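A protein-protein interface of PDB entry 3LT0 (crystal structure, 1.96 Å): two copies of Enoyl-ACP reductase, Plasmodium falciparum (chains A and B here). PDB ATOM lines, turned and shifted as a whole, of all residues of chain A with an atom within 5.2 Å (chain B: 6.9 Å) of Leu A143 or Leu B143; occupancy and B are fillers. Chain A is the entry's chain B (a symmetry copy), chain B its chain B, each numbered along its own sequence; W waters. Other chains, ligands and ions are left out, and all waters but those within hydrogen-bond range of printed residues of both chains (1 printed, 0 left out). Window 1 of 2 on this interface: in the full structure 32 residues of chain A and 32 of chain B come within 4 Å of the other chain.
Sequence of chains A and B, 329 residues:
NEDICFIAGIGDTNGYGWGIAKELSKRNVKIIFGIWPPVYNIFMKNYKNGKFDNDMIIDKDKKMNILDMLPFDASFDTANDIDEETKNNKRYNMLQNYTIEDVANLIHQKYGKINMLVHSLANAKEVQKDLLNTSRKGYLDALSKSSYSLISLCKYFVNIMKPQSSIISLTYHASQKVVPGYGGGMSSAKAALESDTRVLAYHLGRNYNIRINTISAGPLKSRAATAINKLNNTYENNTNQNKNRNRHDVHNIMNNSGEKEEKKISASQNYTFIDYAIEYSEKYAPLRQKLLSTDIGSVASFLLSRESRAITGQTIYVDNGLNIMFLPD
The side-chain hydroxyl of Tyr A139 sits at hydrogen-bond distance from the side-chain carboxylate of Asp B196.
The guanidinium group of Arg B136 sits at hydrogen-bond distance from the side-chain hydroxyl of Ser A144, at 2.9 Å.
OD1 of Asp B196 sits at hydrogen-bond distance from OG of Ser A188 (2.5 Å).
The backbone NH (N) of Arg B136 sits at hydrogen-bond distance from the side-chain hydroxyl (OH) of Tyr A148 (3.2 Å).
The backbone carbonyl oxygen (O) of Ser B144 lies within hydrogen-bond range of the backbone NH (N) of Ser B149, at 3.2 Å.
The side-chain hydroxyl (OG) of Ser A147 is in hydrogen-bond range of the backbone carbonyl oxygen (O) of Ala A189 (2.7 Å).
The backbone NH of Tyr B148 sits at hydrogen-bond distance from the backbone carbonyl oxygen of Leu B143 (2.8 Å).
The backbone NH (N) of Tyr A148 sits at hydrogen-bond distance from the backbone carbonyl oxygen (O) of Leu A143, at 2.8 Å.
OG of Ser B147 is in hydrogen-bond range of O of Ala B189 (2.7 Å).
The backbone carbonyl oxygen of Ser A144 lies within hydrogen-bond range of the backbone NH of Ser A149 (3.2 Å).
Among the printed residues, merely in contact across the chains: Leu A140 with Leu B140, Tyr A139 with Tyr B148, Tyr A148 with Tyr B139, Ser A147 with Tyr B139, Tyr A139 with Ser B147, Ala A192 with Tyr B139, Tyr A139 with Ala B192, Ser A144 with Leu B140, Leu A140 with Ser B144 and Leu A143 with Leu B143.
Of the printed residues of chain B, Leu A143 touches Leu B143.
Printed residues of chain A within 4 Å of Leu B143: Leu A143 (3.9 Å).
Of the printed residues of chain B, Leu A140 touches Leu B140 (3.5 Å) and Ser B144 (3.7 Å).
Printed residues of chain A within 4 Å of Leu B140: Leu A140 and Ser A144.
Ser B187 touches none of the printed residues of chain A.
Leu B150 touches none of the printed residues of chain A.
Of the 15 printed residues of chain A, 8 touch a printed residue of chain B.
Along chain A the printed residues that touch a printed residue of chain B span positions 139 to 192.
Hydrophobic or aromatic side chains of chain B that line the printed part of chain A: Tyr B139, Leu B140, Leu B143, Tyr B148 and Ala B192.
Among the printed residues, 14 pairs touch across the chains.
Among the printed residues, no Asp or Glu carboxylate lies within 4 Å of a Lys or Arg side-chain nitrogen of the other chain.
Tyr A139 touches Tyr B148, and with the chains exchanged Tyr A148 touches Tyr B139.
Tyr A139 touches Ala B192, and with the chains exchanged Ala A192 touches Tyr B139.
Leu B140 touches its own counterpart, Leu A140.
Leu A140 touches Ser B144, and with the chains exchanged Ser A144 touches Leu B140.
Positions printed for both chains: 139, 140, 141, 142, 143, 144, 145, 146, 147, 148, 149, 185, 188, 189 and 192.
Water W1 lies within hydrogen-bond range of the backbone NH (N) of Arg B136 (2.7 Å) and the side-chain hydroxyl (OH) of Tyr A148 (3.3 Å).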
ATOM      1  N   TYR A 139     -20.242 -18.517 -20.466  1.00  0.00           N
ATOM      2  CA  TYR A 139     -19.308 -17.873 -19.518  1.00  0.00           C
ATOM      3  C   TYR A 139     -18.967 -16.456 -19.973  1.00  0.00           C
ATOM      4  O   TYR A 139     -19.029 -15.499 -19.191  1.00  0.00           O
ATOM      5  CB  TYR A 139     -18.030 -18.713 -19.461  1.00  0.00           C
ATOM      6  CG  TYR A 139     -16.953 -18.294 -18.505  1.00  0.00           C
ATOM      7  CD1 TYR A 139     -15.891 -17.497 -18.928  1.00  0.00           C
ATOM      8  CD2 TYR A 139     -16.963 -18.754 -17.162  1.00  0.00           C
ATOM      9  CE1 TYR A 139     -14.842 -17.150 -18.033  1.00  0.00           C
ATOM     10  CE2 TYR A 139     -15.949 -18.429 -16.294  1.00  0.00           C
ATOM     11  CZ  TYR A 139     -14.878 -17.626 -16.727  1.00  0.00           C
ATOM     12  OH  TYR A 139     -13.879 -17.340 -15.841  1.00  0.00           O
ATOM     13  N   LEU A 140     -18.631 -16.319 -21.253  1.00  0.00           N
ATOM     14  CA  LEU A 140     -18.333 -14.985 -21.814  1.00  0.00           C
ATOM     15  C   LEU A 140     -19.529 -14.066 -21.780  1.00  0.00           C
ATOM     16  O   LEU A 140     -19.369 -12.867 -21.566  1.00  0.00           O
ATOM     17  CB  LEU A 140     -17.732 -15.078 -23.230  1.00  0.00           C
ATOM     18  CG  LEU A 140     -16.366 -15.801 -23.275  1.00  0.00           C
ATOM     19  CD1 LEU A 140     -15.918 -15.936 -24.764  1.00  0.00           C
ATOM     20  CD2 LEU A 140     -15.246 -15.098 -22.379  1.00  0.00           C
ATOM     21  N   ASP A 141     -20.733 -14.616 -21.940  1.00  0.00           N
ATOM     22  CA  ASP A 141     -21.940 -13.798 -21.829  1.00  0.00           C
ATOM     23  C   ASP A 141     -22.040 -13.214 -20.408  1.00  0.00           C
ATOM     24  O   ASP A 141     -22.324 -12.028 -20.237  1.00  0.00           O
ATOM     25  CB  ASP A 141     -23.194 -14.650 -22.125  1.00  0.00           C
ATOM     26  CG  ASP A 141     -24.461 -13.848 -22.008  1.00  0.00           C
ATOM     27  OD1 ASP A 141     -25.204 -14.062 -21.038  1.00  0.00           O
ATOM     28  OD2 ASP A 141     -24.677 -12.965 -22.867  1.00  0.00           O
ATOM     29  N   ALA A 142     -21.778 -14.045 -19.393  1.00  0.00           N
ATOM     30  CA  ALA A 142     -21.893 -13.603 -17.999  1.00  0.00           C
ATOM     31  C   ALA A 142     -20.865 -12.467 -17.726  1.00  0.00           C
ATOM     32  O   ALA A 142     -21.199 -11.428 -17.130  1.00  0.00           O
ATOM     33  CB  ALA A 142     -21.684 -14.769 -17.074  1.00  0.00           C
ATOM     34  N   LEU A 143     -19.647 -12.636 -18.229  1.00  0.00           N
ATOM     35  CA  LEU A 143     -18.577 -11.636 -18.013  1.00  0.00           C
ATOM     36  C   LEU A 143     -18.907 -10.365 -18.780  1.00  0.00           C
ATOM     37  O   LEU A 143     -18.713  -9.256 -18.279  1.00  0.00           O
ATOM     38  CB  LEU A 143     -17.217 -12.201 -18.458  1.00  0.00           C
ATOM     39  CG  LEU A 143     -16.437 -12.975 -17.382  1.00  0.00           C
ATOM     40  CD1 LEU A 143     -15.938 -12.007 -16.306  1.00  0.00           C
ATOM     41  CD2 LEU A 143     -17.236 -14.150 -16.712  1.00  0.00           C
ATOM     42  N   SER A 144     -19.425 -10.540 -19.995  1.00  0.00           N
ATOM     43  CA  SER A 144     -19.763  -9.382 -20.848  1.00  0.00           C
ATOM     44  C   SER A 144     -20.799  -8.470 -20.214  1.00  0.00           C
ATOM     45  O   SER A 144     -20.585  -7.248 -20.063  1.00  0.00           O
ATOM     46  CB  SER A 144     -20.237  -9.852 -22.243  1.00  0.00           C
ATOM     47  OG  SER A 144     -20.398  -8.721 -23.088  1.00  0.00           O
ATOM     48  N   LYS A 145     -21.927  -9.052 -19.830  1.00  0.00           N
ATOM     49  CA  LYS A 145     -23.040  -8.275 -19.310  1.00  0.00           C
ATOM     50  C   LYS A 145     -22.842  -7.875 -17.853  1.00  0.00           C
ATOM     51  O   LYS A 145     -23.322  -6.833 -17.443  1.00  0.00           O
ATOM     52  CB  LYS A 145     -24.343  -9.086 -19.355  1.00  0.00           C
ATOM     53  CG  LYS A 145     -24.587  -9.903 -20.640  1.00  0.00           C
ATOM     54  CD  LYS A 145     -25.251  -9.110 -21.681  1.00  0.00           C
ATOM     55  CE  LYS A 145     -26.206 -10.015 -22.512  1.00  0.00           C
ATOM     56  NZ  LYS A 145     -25.558 -10.446 -23.745  1.00  0.00           N
ATOM     57  N   SER A 146     -22.205  -8.724 -17.055  1.00  0.00           N
ATOM     58  CA  SER A 146     -22.170  -8.463 -15.602  1.00  0.00           C
ATOM     59  C   SER A 146     -20.936  -7.727 -15.129  1.00  0.00           C
ATOM     60  O   SER A 146     -20.984  -7.082 -14.060  1.00  0.00           O
ATOM     61  CB  SER A 146     -22.282  -9.753 -14.787  1.00  0.00           C
ATOM     62  OG  SER A 146     -23.423 -10.529 -15.129  1.00  0.00           O
ATOM     63  N   SER A 147     -19.831  -7.851 -15.869  1.00  0.00           N
ATOM     64  CA  SER A 147     -18.545  -7.283 -15.419  1.00  0.00           C
ATOM     65  C   SER A 147     -18.034  -6.232 -16.399  1.00  0.00           C
ATOM     66  O   SER A 147     -17.783  -5.077 -15.993  1.00  0.00           O
ATOM     67  CB  SER A 147     -17.482  -8.374 -15.230  1.00  0.00           C
ATOM     68  OG  SER A 147     -18.062  -9.473 -14.537  1.00  0.00           O
ATOM     69  N   TYR A 148     -17.878  -6.608 -17.672  1.00  0.00           N
ATOM     70  CA  TYR A 148     -17.370  -5.627 -18.635  1.00  0.00           C
ATOM     71  C   TYR A 148     -18.272  -4.376 -18.685  1.00  0.00           C
ATOM     72  O   TYR A 148     -17.784  -3.254 -18.895  1.00  0.00           O
ATOM     73  CB  TYR A 148     -17.128  -6.186 -20.069  1.00  0.00           C
ATOM     74  CG  TYR A 148     -16.491  -5.099 -20.911  1.00  0.00           C
ATOM     75  CD1 TYR A 148     -15.126  -4.808 -20.800  1.00  0.00           C
ATOM     76  CD2 TYR A 148     -17.275  -4.279 -21.721  1.00  0.00           C
ATOM     77  CE1 TYR A 148     -14.554  -3.720 -21.505  1.00  0.00           C
ATOM     78  CE2 TYR A 148     -16.720  -3.218 -22.437  1.00  0.00           C
ATOM     79  CZ  TYR A 148     -15.367  -2.946 -22.326  1.00  0.00           C
ATOM     80  OH  TYR A 148     -14.826  -1.904 -23.055  1.00  0.00           O
ATOM     81  N   SER A 149     -19.582  -4.577 -18.553  1.00  0.00           N
ATOM     82  CA  SER A 149     -20.533  -3.461 -18.603  1.00  0.00           C
ATOM     83  C   SER A 149     -20.145  -2.333 -17.614  1.00  0.00           C
ATOM     84  O   SER A 149     -20.360  -1.151 -17.882  1.00  0.00           O
ATOM     85  CB  SER A 149     -21.930  -3.956 -18.289  1.00  0.00           C
ATOM     86  OG  SER A 149     -21.971  -4.655 -17.072  1.00  0.00           O
ATOM     87  N   GLY A 185     -21.093 -19.012 -14.562  1.00  0.00           N
ATOM     88  CA  GLY A 185     -19.970 -18.054 -14.566  1.00  0.00           C
ATOM     89  C   GLY A 185     -20.330 -16.763 -13.832  1.00  0.00           C
ATOM     90  O   GLY A 185     -19.549 -15.818 -13.866  1.00  0.00           O
ATOM     91  N   SER A 188     -17.688 -16.110 -11.348  1.00  0.00           N
ATOM     92  CA  SER A 188     -16.500 -15.604 -12.052  1.00  0.00           C
ATOM     93  C   SER A 188     -16.670 -14.129 -12.352  1.00  0.00           C
ATOM     94  O   SER A 188     -15.770 -13.336 -12.095  1.00  0.00           O
ATOM     95  CB  SER A 188     -16.308 -16.376 -13.358  1.00  0.00           C
ATOM     96  OG  SER A 188     -16.699 -17.737 -13.187  1.00  0.00           O
ATOM     97  N   ALA A 189     -17.843 -13.760 -12.858  1.00  0.00           N
ATOM     98  CA  ALA A 189     -18.131 -12.374 -13.165  1.00  0.00           C
ATOM     99  C   ALA A 189     -18.031 -11.440 -11.932  1.00  0.00           C
ATOM    100  O   ALA A 189     -17.565 -10.303 -12.046  1.00  0.00           O
ATOM    101  CB  ALA A 189     -19.499 -12.259 -13.826  1.00  0.00           C
ATOM    102  N   ALA A 192     -14.417 -10.959 -10.998  1.00  0.00           N
ATOM    103  CA  ALA A 192     -13.864  -9.984 -11.928  1.00  0.00           C
ATOM    104  C   ALA A 192     -14.298  -8.535 -11.587  1.00  0.00           C
ATOM    105  O   ALA A 192     -13.472  -7.630 -11.549  1.00  0.00           O
ATOM    106  CB  ALA A 192     -14.291 -10.350 -13.374  1.00  0.00           C
ATOM    107  N   ASN B 123      -3.413 -15.425 -22.312  1.00  0.00           N
ATOM    108  CA  ASN B 123      -3.337 -14.559 -23.477  1.00  0.00           C
ATOM    109  C   ASN B 123      -4.386 -13.483 -23.418  1.00  0.00           C
ATOM    110  O   ASN B 123      -5.439 -13.665 -22.810  1.00  0.00           O
ATOM    111  CB  ASN B 123      -3.468 -15.371 -24.771  1.00  0.00           C
ATOM    112  CG  ASN B 123      -2.360 -15.022 -25.762  1.00  0.00           C
ATOM    113  OD1 ASN B 123      -1.857 -15.887 -26.478  1.00  0.00           O
ATOM    114  ND2 ASN B 123      -1.947 -13.748 -25.770  1.00  0.00           N
ATOM    115  N   ALA B 124      -4.086 -12.342 -24.024  1.00  0.00           N
ATOM    116  CA  ALA B 124      -4.980 -11.184 -24.004  1.00  0.00           C
ATOM    117  C   ALA B 124      -4.547 -10.250 -25.130  1.00  0.00           C
ATOM    118  O   ALA B 124      -3.442  -9.715 -25.105  1.00  0.00           O
ATOM    119  CB  ALA B 124      -4.887 -10.455 -22.661  1.00  0.00           C
ATOM    120  N   ARG B 136     -14.539  -4.297 -25.199  1.00  0.00           N
ATOM    121  CA  ARG B 136     -15.307  -5.483 -24.848  1.00  0.00           C
ATOM    122  C   ARG B 136     -14.654  -6.736 -25.437  1.00  0.00           C
ATOM    123  O   ARG B 136     -14.485  -7.737 -24.750  1.00  0.00           O
ATOM    124  CB  ARG B 136     -16.780  -5.345 -25.291  1.00  0.00           C
ATOM    125  CG  ARG B 136     -17.716  -6.488 -24.772  1.00  0.00           C
ATOM    126  CD  ARG B 136     -19.193  -6.229 -25.114  1.00  0.00           C
ATOM    127  NE  ARG B 136     -19.656  -4.942 -24.567  1.00  0.00           N
ATOM    128  CZ  ARG B 136     -20.417  -4.794 -23.483  1.00  0.00           C
ATOM    129  NH1 ARG B 136     -20.827  -5.853 -22.779  1.00  0.00           N
ATOM    130  NH2 ARG B 136     -20.766  -3.571 -23.085  1.00  0.00           N
ATOM    131  N   GLY B 138     -11.505  -7.217 -26.494  1.00  0.00           N
ATOM    132  CA  GLY B 138     -10.227  -7.482 -25.831  1.00  0.00           C
ATOM    133  C   GLY B 138     -10.440  -8.148 -24.468  1.00  0.00           C
ATOM    134  O   GLY B 138      -9.773  -9.133 -24.133  1.00  0.00           O
ATOM    135  N   TYR B 139     -11.359  -7.603 -23.676  1.00  0.00           N
ATOM    136  CA  TYR B 139     -11.607  -8.124 -22.316  1.00  0.00           C
ATOM    137  C   TYR B 139     -12.101  -9.568 -22.373  1.00  0.00           C
ATOM    138  O   TYR B 139     -11.595 -10.449 -21.665  1.00  0.00           O
ATOM    139  CB  TYR B 139     -12.672  -7.247 -21.652  1.00  0.00           C
ATOM    140  CG  TYR B 139     -13.040  -7.543 -20.229  1.00  0.00           C
ATOM    141  CD1 TYR B 139     -14.138  -8.345 -19.926  1.00  0.00           C
ATOM    142  CD2 TYR B 139     -12.313  -6.956 -19.159  1.00  0.00           C
ATOM    143  CE1 TYR B 139     -14.520  -8.576 -18.576  1.00  0.00           C
ATOM    144  CE2 TYR B 139     -12.681  -7.168 -17.853  1.00  0.00           C
ATOM    145  CZ  TYR B 139     -13.792  -7.978 -17.553  1.00  0.00           C
ATOM    146  OH  TYR B 139     -14.138  -8.150 -16.244  1.00  0.00           O
ATOM    147  N   LEU B 140     -13.076  -9.818 -23.244  1.00  0.00           N
ATOM    148  CA  LEU B 140     -13.594 -11.190 -23.421  1.00  0.00           C
ATOM    149  C   LEU B 140     -12.546 -12.136 -23.956  1.00  0.00           C
ATOM    150  O   LEU B 140     -12.529 -13.305 -23.577  1.00  0.00           O
ATOM    151  CB  LEU B 140     -14.871 -11.216 -24.282  1.00  0.00           C
ATOM    152  CG  LEU B 140     -16.062 -10.462 -23.644  1.00  0.00           C
ATOM    153  CD1 LEU B 140     -17.252 -10.458 -24.653  1.00  0.00           C
ATOM    154  CD2 LEU B 140     -16.491 -11.044 -22.221  1.00  0.00           C
ATOM    155  N   ASP B 141     -11.640 -11.638 -24.798  1.00  0.00           N
ATOM    156  CA  ASP B 141     -10.544 -12.476 -25.286  1.00  0.00           C
ATOM    157  C   ASP B 141      -9.670 -12.925 -24.101  1.00  0.00           C
ATOM    158  O   ASP B 141      -9.306 -14.095 -24.000  1.00  0.00           O
ATOM    159  CB  ASP B 141      -9.679 -11.692 -26.297  1.00  0.00           C
ATOM    160  CG  ASP B 141      -8.532 -12.514 -26.813  1.00  0.00           C
ATOM    161  OD1 ASP B 141      -7.387 -12.230 -26.431  1.00  0.00           O
ATOM    162  OD2 ASP B 141      -8.794 -13.482 -27.563  1.00  0.00           O
ATOM    163  N   ALA B 142      -9.360 -11.992 -23.192  1.00  0.00           N
ATOM    164  CA  ALA B 142      -8.491 -12.303 -22.051  1.00  0.00           C
ATOM    165  C   ALA B 142      -9.172 -13.378 -21.154  1.00  0.00           C
ATOM    166  O   ALA B 142      -8.538 -14.363 -20.740  1.00  0.00           O
ATOM    167  CB  ALA B 142      -8.195 -11.048 -21.278  1.00  0.00           C
ATOM    168  N   LEU B 143     -10.472 -13.222 -20.927  1.00  0.00           N
ATOM    169  CA  LEU B 143     -11.222 -14.166 -20.067  1.00  0.00           C
ATOM    170  C   LEU B 143     -11.328 -15.514 -20.765  1.00  0.00           C
ATOM    171  O   LEU B 143     -11.186 -16.564 -20.135  1.00  0.00           O
ATOM    172  CB  LEU B 143     -12.621 -13.609 -19.751  1.00  0.00           C
ATOM    173  CG  LEU B 143     -12.709 -12.712 -18.504  1.00  0.00           C
ATOM    174  CD1 LEU B 143     -12.514 -13.559 -17.243  1.00  0.00           C
ATOM    175  CD2 LEU B 143     -11.709 -11.502 -18.493  1.00  0.00           C
ATOM    176  N   SER B 144     -11.560 -15.471 -22.076  1.00  0.00           N
ATOM    177  CA  SER B 144     -11.709 -16.713 -22.860  1.00  0.00           C
ATOM    178  C   SER B 144     -10.469 -17.591 -22.809  1.00  0.00           C
ATOM    179  O   SER B 144     -10.532 -18.786 -22.450  1.00  0.00           O
ATOM    180  CB  SER B 144     -12.086 -16.393 -24.326  1.00  0.00           C
ATOM    181  OG  SER B 144     -12.379 -17.604 -25.009  1.00  0.00           O
ATOM    182  N   LYS B 145      -9.331 -17.007 -23.160  1.00  0.00           N
ATOM    183  CA  LYS B 145      -8.094 -17.761 -23.259  1.00  0.00           C
ATOM    184  C   LYS B 145      -7.454 -18.015 -21.899  1.00  0.00           C
ATOM    185  O   LYS B 145      -6.799 -19.026 -21.719  1.00  0.00           O
ATOM    186  CB  LYS B 145      -7.049 -16.996 -24.084  1.00  0.00           C
ATOM    187  CG  LYS B 145      -7.568 -16.312 -25.365  1.00  0.00           C
ATOM    188  CD  LYS B 145      -7.557 -17.220 -26.519  1.00  0.00           C
ATOM    189  CE  LYS B 145      -7.236 -16.426 -27.818  1.00  0.00           C
ATOM    190  NZ  LYS B 145      -8.462 -16.098 -28.533  1.00  0.00           N
ATOM    191  N   SER B 146      -7.577 -17.076 -20.968  1.00  0.00           N
ATOM    192  CA  SER B 146      -6.807 -17.195 -19.714  1.00  0.00           C
ATOM    193  C   SER B 146      -7.563 -17.847 -18.577  1.00  0.00           C
ATOM    194  O   SER B 146      -6.922 -18.388 -17.651  1.00  0.00           O
ATOM    195  CB  SER B 146      -6.306 -15.836 -19.219  1.00  0.00           C
ATOM    196  OG  SER B 146      -5.558 -15.131 -20.201  1.00  0.00           O
ATOM    197  N   SER B 147      -8.895 -17.763 -18.603  1.00  0.00           N
ATOM    198  CA  SER B 147      -9.712 -18.248 -17.473  1.00  0.00           C
ATOM    199  C   SER B 147     -10.644 -19.373 -17.910  1.00  0.00           C
ATOM    200  O   SER B 147     -10.600 -20.476 -17.325  1.00  0.00           O
ATOM    201  CB  SER B 147     -10.530 -17.115 -16.841  1.00  0.00           C
ATOM    202  OG  SER B 147      -9.699 -15.971 -16.684  1.00  0.00           O
ATOM    203  N   TYR B 148     -11.480 -19.116 -18.922  1.00  0.00           N
ATOM    204  CA  TYR B 148     -12.402 -20.170 -19.353  1.00  0.00           C
ATOM    205  C   TYR B 148     -11.638 -21.445 -19.767  1.00  0.00           C
ATOM    206  O   TYR B 148     -12.129 -22.568 -19.568  1.00  0.00           O
ATOM    207  CB  TYR B 148     -13.402 -19.745 -20.469  1.00  0.00           C
ATOM    208  CG  TYR B 148     -14.364 -20.889 -20.720  1.00  0.00           C
ATOM    209  CD1 TYR B 148     -15.439 -21.129 -19.855  1.00  0.00           C
ATOM    210  CD2 TYR B 148     -14.125 -21.804 -21.743  1.00  0.00           C
ATOM    211  CE1 TYR B 148     -16.272 -22.262 -20.027  1.00  0.00           C
ATOM    212  CE2 TYR B 148     -14.950 -22.912 -21.936  1.00  0.00           C
ATOM    213  CZ  TYR B 148     -16.016 -23.133 -21.080  1.00  0.00           C
ATOM    214  OH  TYR B 148     -16.837 -24.225 -21.292  1.00  0.00           O
ATOM    215  N   SER B 149     -10.474 -21.270 -20.390  1.00  0.00           N
ATOM    216  CA  SER B 149      -9.672 -22.412 -20.844  1.00  0.00           C
ATOM    217  C   SER B 149      -9.427 -23.429 -19.700  1.00  0.00           C
ATOM    218  O   SER B 149      -9.359 -24.637 -19.928  1.00  0.00           O
ATOM    219  CB  SER B 149      -8.345 -21.930 -21.391  1.00  0.00           C
ATOM    220  OG  SER B 149      -7.667 -21.119 -20.466  1.00  0.00           O
ATOM    221  N   LEU B 150      -9.270 -22.929 -18.483  1.00  0.00           N
ATOM    222  CA  LEU B 150      -9.094 -23.821 -17.313  1.00  0.00           C
ATOM    223  C   LEU B 150     -10.338 -24.670 -17.056  1.00  0.00           C
ATOM    224  O   LEU B 150     -10.240 -25.892 -16.846  1.00  0.00           O
ATOM    225  CB  LEU B 150      -8.809 -22.978 -16.072  1.00  0.00           C
ATOM    226  CG  LEU B 150      -8.110 -23.559 -14.844  1.00  0.00           C
ATOM    227  CD1 LEU B 150      -8.671 -23.141 -13.491  1.00  0.00           C
ATOM    228  CD2 LEU B 150      -7.648 -25.007 -14.902  1.00  0.00           C
ATOM    229  N   GLY B 184      -5.423  -4.996 -20.250  1.00  0.00           N
ATOM    230  CA  GLY B 184      -6.168  -5.820 -21.191  1.00  0.00           C
ATOM    231  C   GLY B 184      -7.171  -6.751 -20.560  1.00  0.00           C
ATOM    232  O   GLY B 184      -7.744  -7.599 -21.242  1.00  0.00           O
ATOM    233  N   GLY B 185      -7.443  -6.569 -19.269  1.00  0.00           N
ATOM    234  CA  GLY B 185      -8.359  -7.491 -18.569  1.00  0.00           C
ATOM    235  C   GLY B 185      -7.621  -8.715 -18.031  1.00  0.00           C
ATOM    236  O   GLY B 185      -8.267  -9.636 -17.543  1.00  0.00           O
ATOM    237  N   MET B 186      -6.281  -8.741 -18.102  1.00  0.00           N
ATOM    238  CA  MET B 186      -5.519  -9.834 -17.471  1.00  0.00           C
ATOM    239  C   MET B 186      -5.740  -9.895 -15.944  1.00  0.00           C
ATOM    240  O   MET B 186      -5.805 -10.981 -15.364  1.00  0.00           O
ATOM    241  CB  MET B 186      -4.007  -9.771 -17.800  1.00  0.00           C
ATOM    242  CG  MET B 186      -3.639 -10.361 -19.185  1.00  0.00           C
ATOM    243  SD  MET B 186      -4.255 -12.074 -19.420  1.00  0.00           S
ATOM    244  CE  MET B 186      -3.711 -12.928 -17.932  1.00  0.00           C
ATOM    245  N   SER B 187      -5.846  -8.740 -15.299  1.00  0.00           N
ATOM    246  CA  SER B 187      -6.123  -8.723 -13.873  1.00  0.00           C
ATOM    247  C   SER B 187      -7.504  -9.372 -13.595  1.00  0.00           C
ATOM    248  O   SER B 187      -7.680 -10.168 -12.655  1.00  0.00           O
ATOM    249  CB  SER B 187      -6.072  -7.285 -13.367  1.00  0.00           C
ATOM    250  OG  SER B 187      -7.057  -6.462 -14.025  1.00  0.00           O
ATOM    251  N   SER B 188      -8.462  -9.052 -14.459  1.00  0.00           N
ATOM    252  CA  SER B 188      -9.827  -9.589 -14.349  1.00  0.00           C
ATOM    253  C   SER B 188      -9.806 -11.090 -14.551  1.00  0.00           C
ATOM    254  O   SER B 188     -10.397 -11.829 -13.771  1.00  0.00           O
ATOM    255  CB  SER B 188     -10.722  -8.940 -15.406  1.00  0.00           C
ATOM    256  OG  SER B 188     -10.339  -7.581 -15.607  1.00  0.00           O
ATOM    257  N   ALA B 189      -9.088 -11.540 -15.577  1.00  0.00           N
ATOM    258  CA  ALA B 189      -8.975 -12.956 -15.857  1.00  0.00           C
ATOM    259  C   ALA B 189      -8.361 -13.765 -14.686  1.00  0.00           C
ATOM    260  O   ALA B 189      -8.781 -14.893 -14.419  1.00  0.00           O
ATOM    261  CB  ALA B 189      -8.186 -13.173 -17.142  1.00  0.00           C
ATOM    262  N   LYS B 190      -7.330 -13.212 -14.049  1.00  0.00           N
ATOM    263  CA  LYS B 190      -6.667 -13.883 -12.942  1.00  0.00           C
ATOM    264  C   LYS B 190      -7.613 -13.906 -11.727  1.00  0.00           C
ATOM    265  O   LYS B 190      -7.648 -14.910 -11.022  1.00  0.00           O
ATOM    266  CB  LYS B 190      -5.354 -13.160 -12.600  1.00  0.00           C
ATOM    267  CG  LYS B 190      -4.217 -13.377 -13.658  1.00  0.00           C
ATOM    268  CD  LYS B 190      -4.160 -14.851 -14.167  1.00  0.00           C
ATOM    269  CE  LYS B 190      -2.864 -15.048 -15.003  1.00  0.00           C
ATOM    270  NZ  LYS B 190      -2.539 -16.449 -15.419  1.00  0.00           N
ATOM    271  N   ALA B 192     -10.866 -14.052 -11.893  1.00  0.00           N
ATOM    272  CA  ALA B 192     -11.809 -15.094 -12.273  1.00  0.00           C
ATOM    273  C   ALA B 192     -11.218 -16.515 -12.086  1.00  0.00           C
ATOM    274  O   ALA B 192     -11.864 -17.389 -11.519  1.00  0.00           O
ATOM    275  CB  ALA B 192     -12.249 -14.880 -13.745  1.00  0.00           C
ATOM    276  N   LEU B 193      -9.991 -16.709 -12.552  1.00  0.00           N
ATOM    277  CA  LEU B 193      -9.293 -17.965 -12.427  1.00  0.00           C
ATOM    278  C   LEU B 193      -9.184 -18.405 -10.967  1.00  0.00           C
ATOM    279  O   LEU B 193      -9.378 -19.601 -10.640  1.00  0.00           O
ATOM    280  CB  LEU B 193      -7.903 -17.848 -13.082  1.00  0.00           C
ATOM    281  CG  LEU B 193      -6.929 -19.031 -13.130  1.00  0.00           C
ATOM    282  CD1 LEU B 193      -7.230 -19.884 -14.316  1.00  0.00           C
ATOM    283  CD2 LEU B 193      -5.516 -18.552 -13.373  1.00  0.00           C
ATOM    284  N   ASP B 196     -12.747 -19.324  -9.811  1.00  0.00           N
ATOM    285  CA  ASP B 196     -13.125 -20.571 -10.477  1.00  0.00           C
ATOM    286  C   ASP B 196     -12.378 -21.774  -9.887  1.00  0.00           C
ATOM    287  O   ASP B 196     -12.898 -22.909  -9.885  1.00  0.00           O
ATOM    288  CB  ASP B 196     -12.849 -20.462 -11.982  1.00  0.00           C
ATOM    289  CG  ASP B 196     -13.741 -19.408 -12.685  1.00  0.00           C
ATOM    290  OD1 ASP B 196     -14.742 -18.901 -12.065  1.00  0.00           O
ATOM    291  OD2 ASP B 196     -13.422 -19.091 -13.869  1.00  0.00           O
HETATM  292  O   HOH W   1     -15.713  -2.097 -26.274  1.00  0.00           O
